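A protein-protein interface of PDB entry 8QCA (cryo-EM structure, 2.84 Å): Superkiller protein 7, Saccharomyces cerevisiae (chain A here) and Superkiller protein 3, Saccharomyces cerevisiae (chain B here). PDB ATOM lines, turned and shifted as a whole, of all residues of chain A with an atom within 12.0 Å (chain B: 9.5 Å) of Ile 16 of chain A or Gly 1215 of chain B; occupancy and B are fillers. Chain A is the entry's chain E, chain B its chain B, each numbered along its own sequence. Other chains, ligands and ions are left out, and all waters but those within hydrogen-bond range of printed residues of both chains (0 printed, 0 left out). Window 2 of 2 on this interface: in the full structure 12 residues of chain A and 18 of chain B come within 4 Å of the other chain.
Of the printed residues of chain B, Ile 16 of chain A touches Gly 1215 and Ile 1216. Gly 1215 of chain B touches one residue of chain A. Of chain A, only Glu 9 (3.8 Å) and Arg 13 (3.8 Å) come within 4 Å of Leu 1212 of chain B. No residue of chain A comes within 4 Å of Ser 1213 of chain B. No residue of chain A comes within 4 Å of Gln 1214 of chain B. No residue of chain A comes within 4 Å of Ile 1217 of chain B. No residue of chain A comes within 4 Å of Ser 1218 of chain B. Of the printed residues of chain A, Ile 1216 of chain B touches Ile 16. Of the printed residues of chain B, Arg 13 of chain A touches Leu 1212 (3.8 Å). Printed residues of chain A within 4 Å of Phe 1186 of chain B: Leu 8 (3.6 Å). Printed residues of chain B within 4 Å of Leu 8 of chain A: Phe 1186 (3.6 Å). Of the printed residues of chain B, Glu 9 of chain A touches Leu 1212. Glu 1208 of chain B touches none of the printed residues of chain A. The nearest residue of chain A that does not touch Gly 1215 of chain B is Arg 15 of chain A (4.8 Å). The nearest printed residue of chain B that does not touch Arg 13 of chain A is Glu 1208 of chain B (4.2 Å).
CD2 of Leu 8 of chain A touches CD1 of Phe 1186 of chain B, 3.6 Å away. Glu 9 of chain A touches Leu 1212 of chain B (OE2 to CD1, 3.8 Å). CD1 of Leu 1212 of chain B touches NH2 of Arg 13 of chain A (3.8 Å). Gly 1215 of chain B touches Ile 16 of chain A (C to CG1, 3.5 Å). Ile 16 of chain A touches Ile 1216 of chain B.
Hydrophobic or aromatic side chains of chain B within 4 Å of the printed part of chain A: Phe 1186 and Leu 1212. Of the 11 printed residues of chain A, 4 touch a printed residue of chain B. Hydrophobic or aromatic side chains of chain A that line the printed part of chain B: Leu 8 and Ile 16. Among the printed residues, no Asp or Glu carboxylate lies within 4 Å of a Lys or Arg side-chain nitrogen of the other chain.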
ATOM      1  N   SER A   6     -14.006 -10.676  11.234  1.00  0.00           N
ATOM      2  CA  SER A   6     -13.666  -9.272  11.071  1.00  0.00           C
ATOM      3  C   SER A   6     -14.896  -8.420  11.353  1.00  0.00           C
ATOM      4  O   SER A   6     -16.031  -8.855  11.142  1.00  0.00           O
ATOM      5  CB  SER A   6     -13.131  -8.977   9.663  1.00  0.00           C
ATOM      6  OG  SER A   6     -12.788  -7.610   9.524  1.00  0.00           O
ATOM      7  N   LEU A   7     -14.654  -7.199  11.833  1.00  0.00           N
ATOM      8  CA  LEU A   7     -15.759  -6.299  12.155  1.00  0.00           C
ATOM      9  C   LEU A   7     -16.545  -5.914  10.907  1.00  0.00           C
ATOM     10  O   LEU A   7     -17.780  -5.874  10.931  1.00  0.00           O
ATOM     11  CB  LEU A   7     -15.230  -5.051  12.861  1.00  0.00           C
ATOM     12  CG  LEU A   7     -14.677  -5.241  14.274  1.00  0.00           C
ATOM     13  CD1 LEU A   7     -14.607  -3.907  15.003  1.00  0.00           C
ATOM     14  CD2 LEU A   7     -15.514  -6.242  15.057  1.00  0.00           C
ATOM     15  N   LEU A   8     -15.844  -5.621   9.809  1.00  0.00           N
ATOM     16  CA  LEU A   8     -16.527  -5.250   8.574  1.00  0.00           C
ATOM     17  C   LEU A   8     -17.362  -6.404   8.036  1.00  0.00           C
ATOM     18  O   LEU A   8     -18.492  -6.201   7.579  1.00  0.00           O
ATOM     19  CB  LEU A   8     -15.513  -4.790   7.528  1.00  0.00           C
ATOM     20  CG  LEU A   8     -16.038  -3.797   6.490  1.00  0.00           C
ATOM     21  CD1 LEU A   8     -16.691  -2.604   7.168  1.00  0.00           C
ATOM     22  CD2 LEU A   8     -14.924  -3.349   5.562  1.00  0.00           C
ATOM     23  N   GLU A   9     -16.821  -7.622   8.081  1.00  0.00           N
ATOM     24  CA  GLU A   9     -17.580  -8.781   7.624  1.00  0.00           C
ATOM     25  C   GLU A   9     -18.796  -9.026   8.509  1.00  0.00           C
ATOM     26  O   GLU A   9     -19.873  -9.378   8.014  1.00  0.00           O
ATOM     27  CB  GLU A   9     -16.681 -10.016   7.585  1.00  0.00           C
ATOM     28  CG  GLU A   9     -17.184 -11.119   6.669  1.00  0.00           C
ATOM     29  CD  GLU A   9     -16.144 -12.193   6.424  1.00  0.00           C
ATOM     30  OE1 GLU A   9     -15.048 -12.106   7.016  1.00  0.00           O
ATOM     31  OE2 GLU A   9     -16.423 -13.123   5.639  1.00  0.00           O
ATOM     32  N   GLN A  10     -18.642  -8.846   9.823  1.00  0.00           N
ATOM     33  CA  GLN A  10     -19.778  -8.999  10.728  1.00  0.00           C
ATOM     34  C   GLN A  10     -20.860  -7.968  10.436  1.00  0.00           C
ATOM     35  O   GLN A  10     -22.052  -8.295  10.426  1.00  0.00           O
ATOM     36  CB  GLN A  10     -19.311  -8.892  12.180  1.00  0.00           C
ATOM     37  CG  GLN A  10     -18.579 -10.123  12.689  1.00  0.00           C
ATOM     38  CD  GLN A  10     -17.686  -9.817  13.876  1.00  0.00           C
ATOM     39  OE1 GLN A  10     -17.723  -8.719  14.430  1.00  0.00           O
ATOM     40  NE2 GLN A  10     -16.874 -10.790  14.272  1.00  0.00           N
ATOM     41  N   LEU A  11     -20.465  -6.715  10.193  1.00  0.00           N
ATOM     42  CA  LEU A  11     -21.443  -5.684   9.859  1.00  0.00           C
ATOM     43  C   LEU A  11     -22.140  -5.992   8.538  1.00  0.00           C
ATOM     44  O   LEU A  11     -23.357  -5.806   8.409  1.00  0.00           O
ATOM     45  CB  LEU A  11     -20.765  -4.316   9.803  1.00  0.00           C
ATOM     46  CG  LEU A  11     -21.664  -3.124   9.470  1.00  0.00           C
ATOM     47  CD1 LEU A  11     -22.831  -3.044  10.443  1.00  0.00           C
ATOM     48  CD2 LEU A  11     -20.865  -1.831   9.477  1.00  0.00           C
ATOM     49  N   ALA A  12     -21.382  -6.462   7.544  1.00  0.00           N
ATOM     50  CA  ALA A  12     -21.977  -6.813   6.260  1.00  0.00           C
ATOM     51  C   ALA A  12     -22.975  -7.955   6.408  1.00  0.00           C
ATOM     52  O   ALA A  12     -24.057  -7.924   5.812  1.00  0.00           O
ATOM     53  CB  ALA A  12     -20.884  -7.180   5.257  1.00  0.00           C
ATOM     54  N   ARG A  13     -22.628  -8.972   7.201  1.00  0.00           N
ATOM     55  CA  ARG A  13     -23.556 -10.072   7.438  1.00  0.00           C
ATOM     56  C   ARG A  13     -24.786  -9.616   8.212  1.00  0.00           C
ATOM     57  O   ARG A  13     -25.890 -10.117   7.970  1.00  0.00           O
ATOM     58  CB  ARG A  13     -22.849 -11.207   8.178  1.00  0.00           C
ATOM     59  CG  ARG A  13     -21.787 -11.911   7.354  1.00  0.00           C
ATOM     60  CD  ARG A  13     -22.414 -12.712   6.226  1.00  0.00           C
ATOM     61  NE  ARG A  13     -21.412 -13.351   5.381  1.00  0.00           N
ATOM     62  CZ  ARG A  13     -20.893 -14.548   5.611  1.00  0.00           C
ATOM     63  NH1 ARG A  13     -21.253 -15.269   6.659  1.00  0.00           N
ATOM     64  NH2 ARG A  13     -19.987 -15.035   4.766  1.00  0.00           N
ATOM     65  N   LYS A  14     -24.616  -8.678   9.149  1.00  0.00           N
ATOM     66  CA  LYS A  14     -25.764  -8.129   9.861  1.00  0.00           C
ATOM     67  C   LYS A  14     -26.696  -7.389   8.911  1.00  0.00           C
ATOM     68  O   LYS A  14     -27.923  -7.501   9.021  1.00  0.00           O
ATOM     69  CB  LYS A  14     -25.292  -7.202  10.981  1.00  0.00           C
ATOM     70  N   ARG A  15     -26.135  -6.631   7.968  1.00  0.00           N
ATOM     71  CA  ARG A  15     -26.962  -5.913   7.005  1.00  0.00           C
ATOM     72  C   ARG A  15     -27.575  -6.825   5.949  1.00  0.00           C
ATOM     73  O   ARG A  15     -28.454  -6.374   5.206  1.00  0.00           O
ATOM     74  CB  ARG A  15     -26.147  -4.811   6.327  1.00  0.00           C
ATOM     75  CG  ARG A  15     -25.689  -3.716   7.274  1.00  0.00           C
ATOM     76  CD  ARG A  15     -26.879  -2.953   7.833  1.00  0.00           C
ATOM     77  NE  ARG A  15     -26.473  -1.848   8.694  1.00  0.00           N
ATOM     78  CZ  ARG A  15     -27.313  -1.109   9.405  1.00  0.00           C
ATOM     79  NH1 ARG A  15     -28.616  -1.329   9.386  1.00  0.00           N
ATOM     80  NH2 ARG A  15     -26.830  -0.120  10.154  1.00  0.00           N
ATOM     81  N   ILE A  16     -27.142  -8.079   5.861  1.00  0.00           N
ATOM     82  CA  ILE A  16     -27.732  -9.023   4.919  1.00  0.00           C
ATOM     83  C   ILE A  16     -29.007  -9.617   5.503  1.00  0.00           C
ATOM     84  O   ILE A  16     -30.006  -8.918   5.674  1.00  0.00           O
ATOM     85  CB  ILE A  16     -26.739 -10.135   4.539  1.00  0.00           C
ATOM     86  CG1 ILE A  16     -25.637  -9.583   3.633  1.00  0.00           C
ATOM     87  CG2 ILE A  16     -27.463 -11.290   3.862  1.00  0.00           C
ATOM     88  CD1 ILE A  16     -24.499 -10.551   3.393  1.00  0.00           C
ATOM     89  N   LEU B1183     -18.727   0.136   2.828  1.00  0.00           N
ATOM     90  CA  LEU B1183     -19.396  -1.085   2.396  1.00  0.00           C
ATOM     91  C   LEU B1183     -19.645  -1.112   0.894  1.00  0.00           C
ATOM     92  O   LEU B1183     -19.847  -2.194   0.333  1.00  0.00           O
ATOM     93  CB  LEU B1183     -20.719  -1.251   3.144  1.00  0.00           C
ATOM     94  N   PHE B1186     -16.454  -2.428  -0.612  1.00  0.00           N
ATOM     95  CA  PHE B1186     -16.261  -3.788  -0.121  1.00  0.00           C
ATOM     96  C   PHE B1186     -16.946  -4.800  -1.031  1.00  0.00           C
ATOM     97  O   PHE B1186     -16.378  -5.853  -1.343  1.00  0.00           O
ATOM     98  CB  PHE B1186     -16.790  -3.893   1.311  1.00  0.00           C
ATOM     99  CG  PHE B1186     -16.336  -5.121   2.044  1.00  0.00           C
ATOM    100  CD1 PHE B1186     -15.022  -5.250   2.459  1.00  0.00           C
ATOM    101  CD2 PHE B1186     -17.228  -6.136   2.344  1.00  0.00           C
ATOM    102  CE1 PHE B1186     -14.602  -6.374   3.142  1.00  0.00           C
ATOM    103  CE2 PHE B1186     -16.815  -7.262   3.027  1.00  0.00           C
ATOM    104  CZ  PHE B1186     -15.499  -7.380   3.427  1.00  0.00           C
ATOM    105  N   ALA B1187     -18.164  -4.488  -1.480  1.00  0.00           N
ATOM    106  CA  ALA B1187     -18.886  -5.391  -2.370  1.00  0.00           C
ATOM    107  C   ALA B1187     -18.176  -5.540  -3.711  1.00  0.00           C
ATOM    108  O   ALA B1187     -18.097  -6.645  -4.260  1.00  0.00           O
ATOM    109  CB  ALA B1187     -20.317  -4.893  -2.573  1.00  0.00           C
ATOM    110  N   LYS B1190     -15.138  -7.681  -3.224  1.00  0.00           N
ATOM    111  CA  LYS B1190     -15.549  -9.072  -3.070  1.00  0.00           C
ATOM    112  C   LYS B1190     -15.941  -9.689  -4.408  1.00  0.00           C
ATOM    113  O   LYS B1190     -15.635 -10.857  -4.670  1.00  0.00           O
ATOM    114  CB  LYS B1190     -16.703  -9.171  -2.072  1.00  0.00           C
ATOM    115  N   ILE B1207     -18.195 -18.848  -4.939  1.00  0.00           N
ATOM    116  CA  ILE B1207     -19.613 -18.783  -4.601  1.00  0.00           C
ATOM    117  C   ILE B1207     -19.816 -18.004  -3.310  1.00  0.00           C
ATOM    118  O   ILE B1207     -20.745 -17.193  -3.198  1.00  0.00           O
ATOM    119  CB  ILE B1207     -20.206 -20.201  -4.504  1.00  0.00           C
ATOM    120  N   GLU B1208     -18.955 -18.234  -2.315  1.00  0.00           N
ATOM    121  CA  GLU B1208     -19.079 -17.522  -1.046  1.00  0.00           C
ATOM    122  C   GLU B1208     -18.923 -16.016  -1.239  1.00  0.00           C
ATOM    123  O   GLU B1208     -19.724 -15.225  -0.727  1.00  0.00           O
ATOM    124  CB  GLU B1208     -18.043 -18.045  -0.050  1.00  0.00           C
ATOM    125  CG  GLU B1208     -18.428 -19.350   0.629  1.00  0.00           C
ATOM    126  CD  GLU B1208     -19.689 -19.229   1.462  1.00  0.00           C
ATOM    127  OE1 GLU B1208     -19.956 -18.128   1.990  1.00  0.00           O
ATOM    128  OE2 GLU B1208     -20.412 -20.238   1.594  1.00  0.00           O
ATOM    129  N   ASN B1209     -17.895 -15.604  -1.985  1.00  0.00           N
ATOM    130  CA  ASN B1209     -17.662 -14.179  -2.195  1.00  0.00           C
ATOM    131  C   ASN B1209     -18.763 -13.550  -3.040  1.00  0.00           C
ATOM    132  O   ASN B1209     -19.169 -12.409  -2.787  1.00  0.00           O
ATOM    133  CB  ASN B1209     -16.295 -13.961  -2.835  1.00  0.00           C
ATOM    134  CG  ASN B1209     -15.164 -14.091  -1.843  1.00  0.00           C
ATOM    135  OD1 ASN B1209     -14.451 -15.094  -1.824  1.00  0.00           O
ATOM    136  ND2 ASN B1209     -14.992 -13.076  -1.006  1.00  0.00           N
ATOM    137  N   ALA B1210     -19.255 -14.270  -4.053  1.00  0.00           N
ATOM    138  CA  ALA B1210     -20.358 -13.752  -4.855  1.00  0.00           C
ATOM    139  C   ALA B1210     -21.612 -13.569  -4.011  1.00  0.00           C
ATOM    140  O   ALA B1210     -22.316 -12.560  -4.142  1.00  0.00           O
ATOM    141  CB  ALA B1210     -20.633 -14.684  -6.033  1.00  0.00           C
ATOM    142  N   ASP B1211     -21.909 -14.534  -3.137  1.00  0.00           N
ATOM    143  CA  ASP B1211     -23.060 -14.402  -2.251  1.00  0.00           C
ATOM    144  C   ASP B1211     -22.896 -13.219  -1.308  1.00  0.00           C
ATOM    145  O   ASP B1211     -23.846 -12.461  -1.080  1.00  0.00           O
ATOM    146  CB  ASP B1211     -23.263 -15.693  -1.461  1.00  0.00           C
ATOM    147  CG  ASP B1211     -23.975 -16.761  -2.262  1.00  0.00           C
ATOM    148  OD1 ASP B1211     -24.747 -16.405  -3.177  1.00  0.00           O
ATOM    149  OD2 ASP B1211     -23.763 -17.959  -1.979  1.00  0.00           O
ATOM    150  N   LEU B1212     -21.695 -13.044  -0.750  1.00  0.00           N
ATOM    151  CA  LEU B1212     -21.456 -11.922   0.154  1.00  0.00           C
ATOM    152  C   LEU B1212     -21.638 -10.590  -0.566  1.00  0.00           C
ATOM    153  O   LEU B1212     -22.277  -9.669  -0.043  1.00  0.00           O
ATOM    154  CB  LEU B1212     -20.054 -12.029   0.755  1.00  0.00           C
ATOM    155  CG  LEU B1212     -19.735 -11.140   1.958  1.00  0.00           C
ATOM    156  CD1 LEU B1212     -18.891 -11.900   2.966  1.00  0.00           C
ATOM    157  CD2 LEU B1212     -19.027  -9.866   1.525  1.00  0.00           C
ATOM    158  N   SER B1213     -21.088 -10.476  -1.777  1.00  0.00           N
ATOM    159  CA  SER B1213     -21.226  -9.244  -2.544  1.00  0.00           C
ATOM    160  C   SER B1213     -22.676  -8.970  -2.918  1.00  0.00           C
ATOM    161  O   SER B1213     -23.122  -7.819  -2.860  1.00  0.00           O
ATOM    162  CB  SER B1213     -20.357  -9.308  -3.800  1.00  0.00           C
ATOM    163  OG  SER B1213     -20.510  -8.145  -4.592  1.00  0.00           O
ATOM    164  N   GLN B1214     -23.421 -10.007  -3.310  1.00  0.00           N
ATOM    165  CA  GLN B1214     -24.828  -9.822  -3.648  1.00  0.00           C
ATOM    166  C   GLN B1214     -25.635  -9.384  -2.432  1.00  0.00           C
ATOM    167  O   GLN B1214     -26.508  -8.516  -2.536  1.00  0.00           O
ATOM    168  CB  GLN B1214     -25.397 -11.113  -4.236  1.00  0.00           C
ATOM    169  CG  GLN B1214     -26.614 -10.912  -5.119  1.00  0.00           C
ATOM    170  CD  GLN B1214     -26.241 -10.552  -6.543  1.00  0.00           C
ATOM    171  OE1 GLN B1214     -25.888 -11.419  -7.342  1.00  0.00           O
ATOM    172  NE2 GLN B1214     -26.316  -9.267  -6.867  1.00  0.00           N
ATOM    173  N   GLY B1215     -25.356  -9.977  -1.269  1.00  0.00           N
ATOM    174  CA  GLY B1215     -26.069  -9.590  -0.063  1.00  0.00           C
ATOM    175  C   GLY B1215     -25.745  -8.178   0.392  1.00  0.00           C
ATOM    176  O   GLY B1215     -26.628  -7.451   0.854  1.00  0.00           O
ATOM    177  N   ILE B1216     -24.478  -7.773   0.274  1.00  0.00           N
ATOM    178  CA  ILE B1216     -24.067  -6.469   0.787  1.00  0.00           C
ATOM    179  C   ILE B1216     -24.740  -5.334   0.024  1.00  0.00           C
ATOM    180  O   ILE B1216     -25.015  -4.272   0.597  1.00  0.00           O
ATOM    181  CB  ILE B1216     -22.534  -6.336   0.747  1.00  0.00           C
ATOM    182  N   ILE B1217     -25.010  -5.521  -1.267  1.00  0.00           N
ATOM    183  CA  ILE B1217     -25.635  -4.478  -2.072  1.00  0.00           C
ATOM    184  C   ILE B1217     -26.701  -5.089  -2.973  1.00  0.00           C
ATOM    185  O   ILE B1217     -26.386  -5.690  -4.006  1.00  0.00           O
ATOM    186  CB  ILE B1217     -24.589  -3.715  -2.903  1.00  0.00           C
ATOM    187  N   SER B1218     -27.961  -4.939  -2.589  1.00  0.00           N
ATOM    188  CA  SER B1218     -29.079  -5.442  -3.381  1.00  0.00           C
ATOM    189  C   SER B1218     -30.123  -4.377  -3.679  1.00  0.00           C
ATOM    190  O   SER B1218     -30.698  -4.379  -4.770  1.00  0.00           O
ATOM    191  CB  SER B1218     -29.742  -6.630  -2.665  1.00  0.00           C
ATOM    192  N   GLU B1219     -30.381  -3.469  -2.742  1.00  0.00           N
ATOM    193  CA  GLU B1219     -31.366  -2.413  -2.928  1.00  0.00           C
ATOM    194  C   GLU B1219     -30.787  -1.167  -3.584  1.00  0.00           C
ATOM    195  O   GLU B1219     -31.541  -0.234  -3.878  1.00  0.00           O
ATOM    196  CB  GLU B1219     -31.998  -2.039  -1.584  1.00  0.00           C
ATOM    197  N   SER B1220     -29.478  -1.126  -3.816  1.00  0.00           N
ATOM    198  CA  SER B1220     -28.863   0.046  -4.421  1.00  0.00           C
ATOM    199  C   SER B1220     -29.217   0.141  -5.900  1.00  0.00           C
ATOM    200  O   SER B1220     -29.382  -0.867  -6.593  1.00  0.00           O
ATOM    201  CB  SER B1220     -27.344   0.000  -4.248  1.00  0.00           C
ATOM    202  N   THR B1228     -21.535  -4.912 -10.889  1.00  0.00           N
ATOM    203  CA  THR B1228     -21.258  -5.889  -9.843  1.00  0.00           C
ATOM    204  C   THR B1228     -22.337  -6.961  -9.788  1.00  0.00           C
ATOM    205  O   THR B1228     -22.034  -8.138  -9.570  1.00  0.00           O
ATOM    206  CB  THR B1228     -21.123  -5.192  -8.490  1.00  0.00           C
ATOM    207  N   LYS B1229     -23.600  -6.579  -9.985  1.00  0.00           N
ATOM    208  CA  LYS B1229     -24.679  -7.563  -9.984  1.00  0.00           C
ATOM    209  C   LYS B1229     -24.511  -8.564 -11.123  1.00  0.00           C
ATOM    210  O   LYS B1229     -24.649  -9.778 -10.926  1.00  0.00           O
ATOM    211  CB  LYS B1229     -26.032  -6.857 -10.085  1.00  0.00           C
ATOM    212  CG  LYS B1229     -26.493  -6.205  -8.794  1.00  0.00           C
ATOM    213  CD  LYS B1229     -27.909  -5.672  -8.930  1.00  0.00           C
ATOM    214  CE  LYS B1229     -28.192  -4.584  -7.910  1.00  0.00           C
ATOM    215  NZ  LYS B1229     -29.408  -3.803  -8.264  1.00  0.00           N
ATOM    216  N   ASN B1232     -21.531 -10.859 -10.373  1.00  0.00           N
ATOM    217  CA  ASN B1232     -21.862 -11.842  -9.351  1.00  0.00           C
ATOM    218  C   ASN B1232     -22.766 -12.932  -9.905  1.00  0.00           C
ATOM    219  O   ASN B1232     -22.599 -14.110  -9.570  1.00  0.00           O
ATOM    220  CB  ASN B1232     -22.514 -11.150  -8.157  1.00  0.00           C
ATOM    221  CG  ASN B1232     -21.546 -10.265  -7.400  1.00  0.00           C
ATOM    222  OD1 ASN B1232     -20.333 -10.464  -7.454  1.00  0.00           O
ATOM    223  ND2 ASN B1232     -22.077  -9.275  -6.693  1.00  0.00           N
ATOM    224  N   LEU B1236     -21.687 -16.823  -9.931  1.00  0.00           N
ATOM    225  CA  LEU B1236     -22.514 -17.815  -9.252  1.00  0.00           C
ATOM    226  C   LEU B1236     -22.942 -18.918 -10.209  1.00  0.00           C
ATOM    227  O   LEU B1236     -22.784 -20.110  -9.914  1.00  0.00           O
ATOM    228  CB  LEU B1236     -23.738 -17.136  -8.637  1.00  0.00           C
ATOM    229  CG  LEU B1236     -23.606 -16.616  -7.206  1.00  0.00           C
ATOM    230  CD1 LEU B1236     -24.605 -15.499  -6.956  1.00  0.00           C
ATOM    231  CD2 LEU B1236     -23.798 -17.740  -6.208  1.00  0.00           C
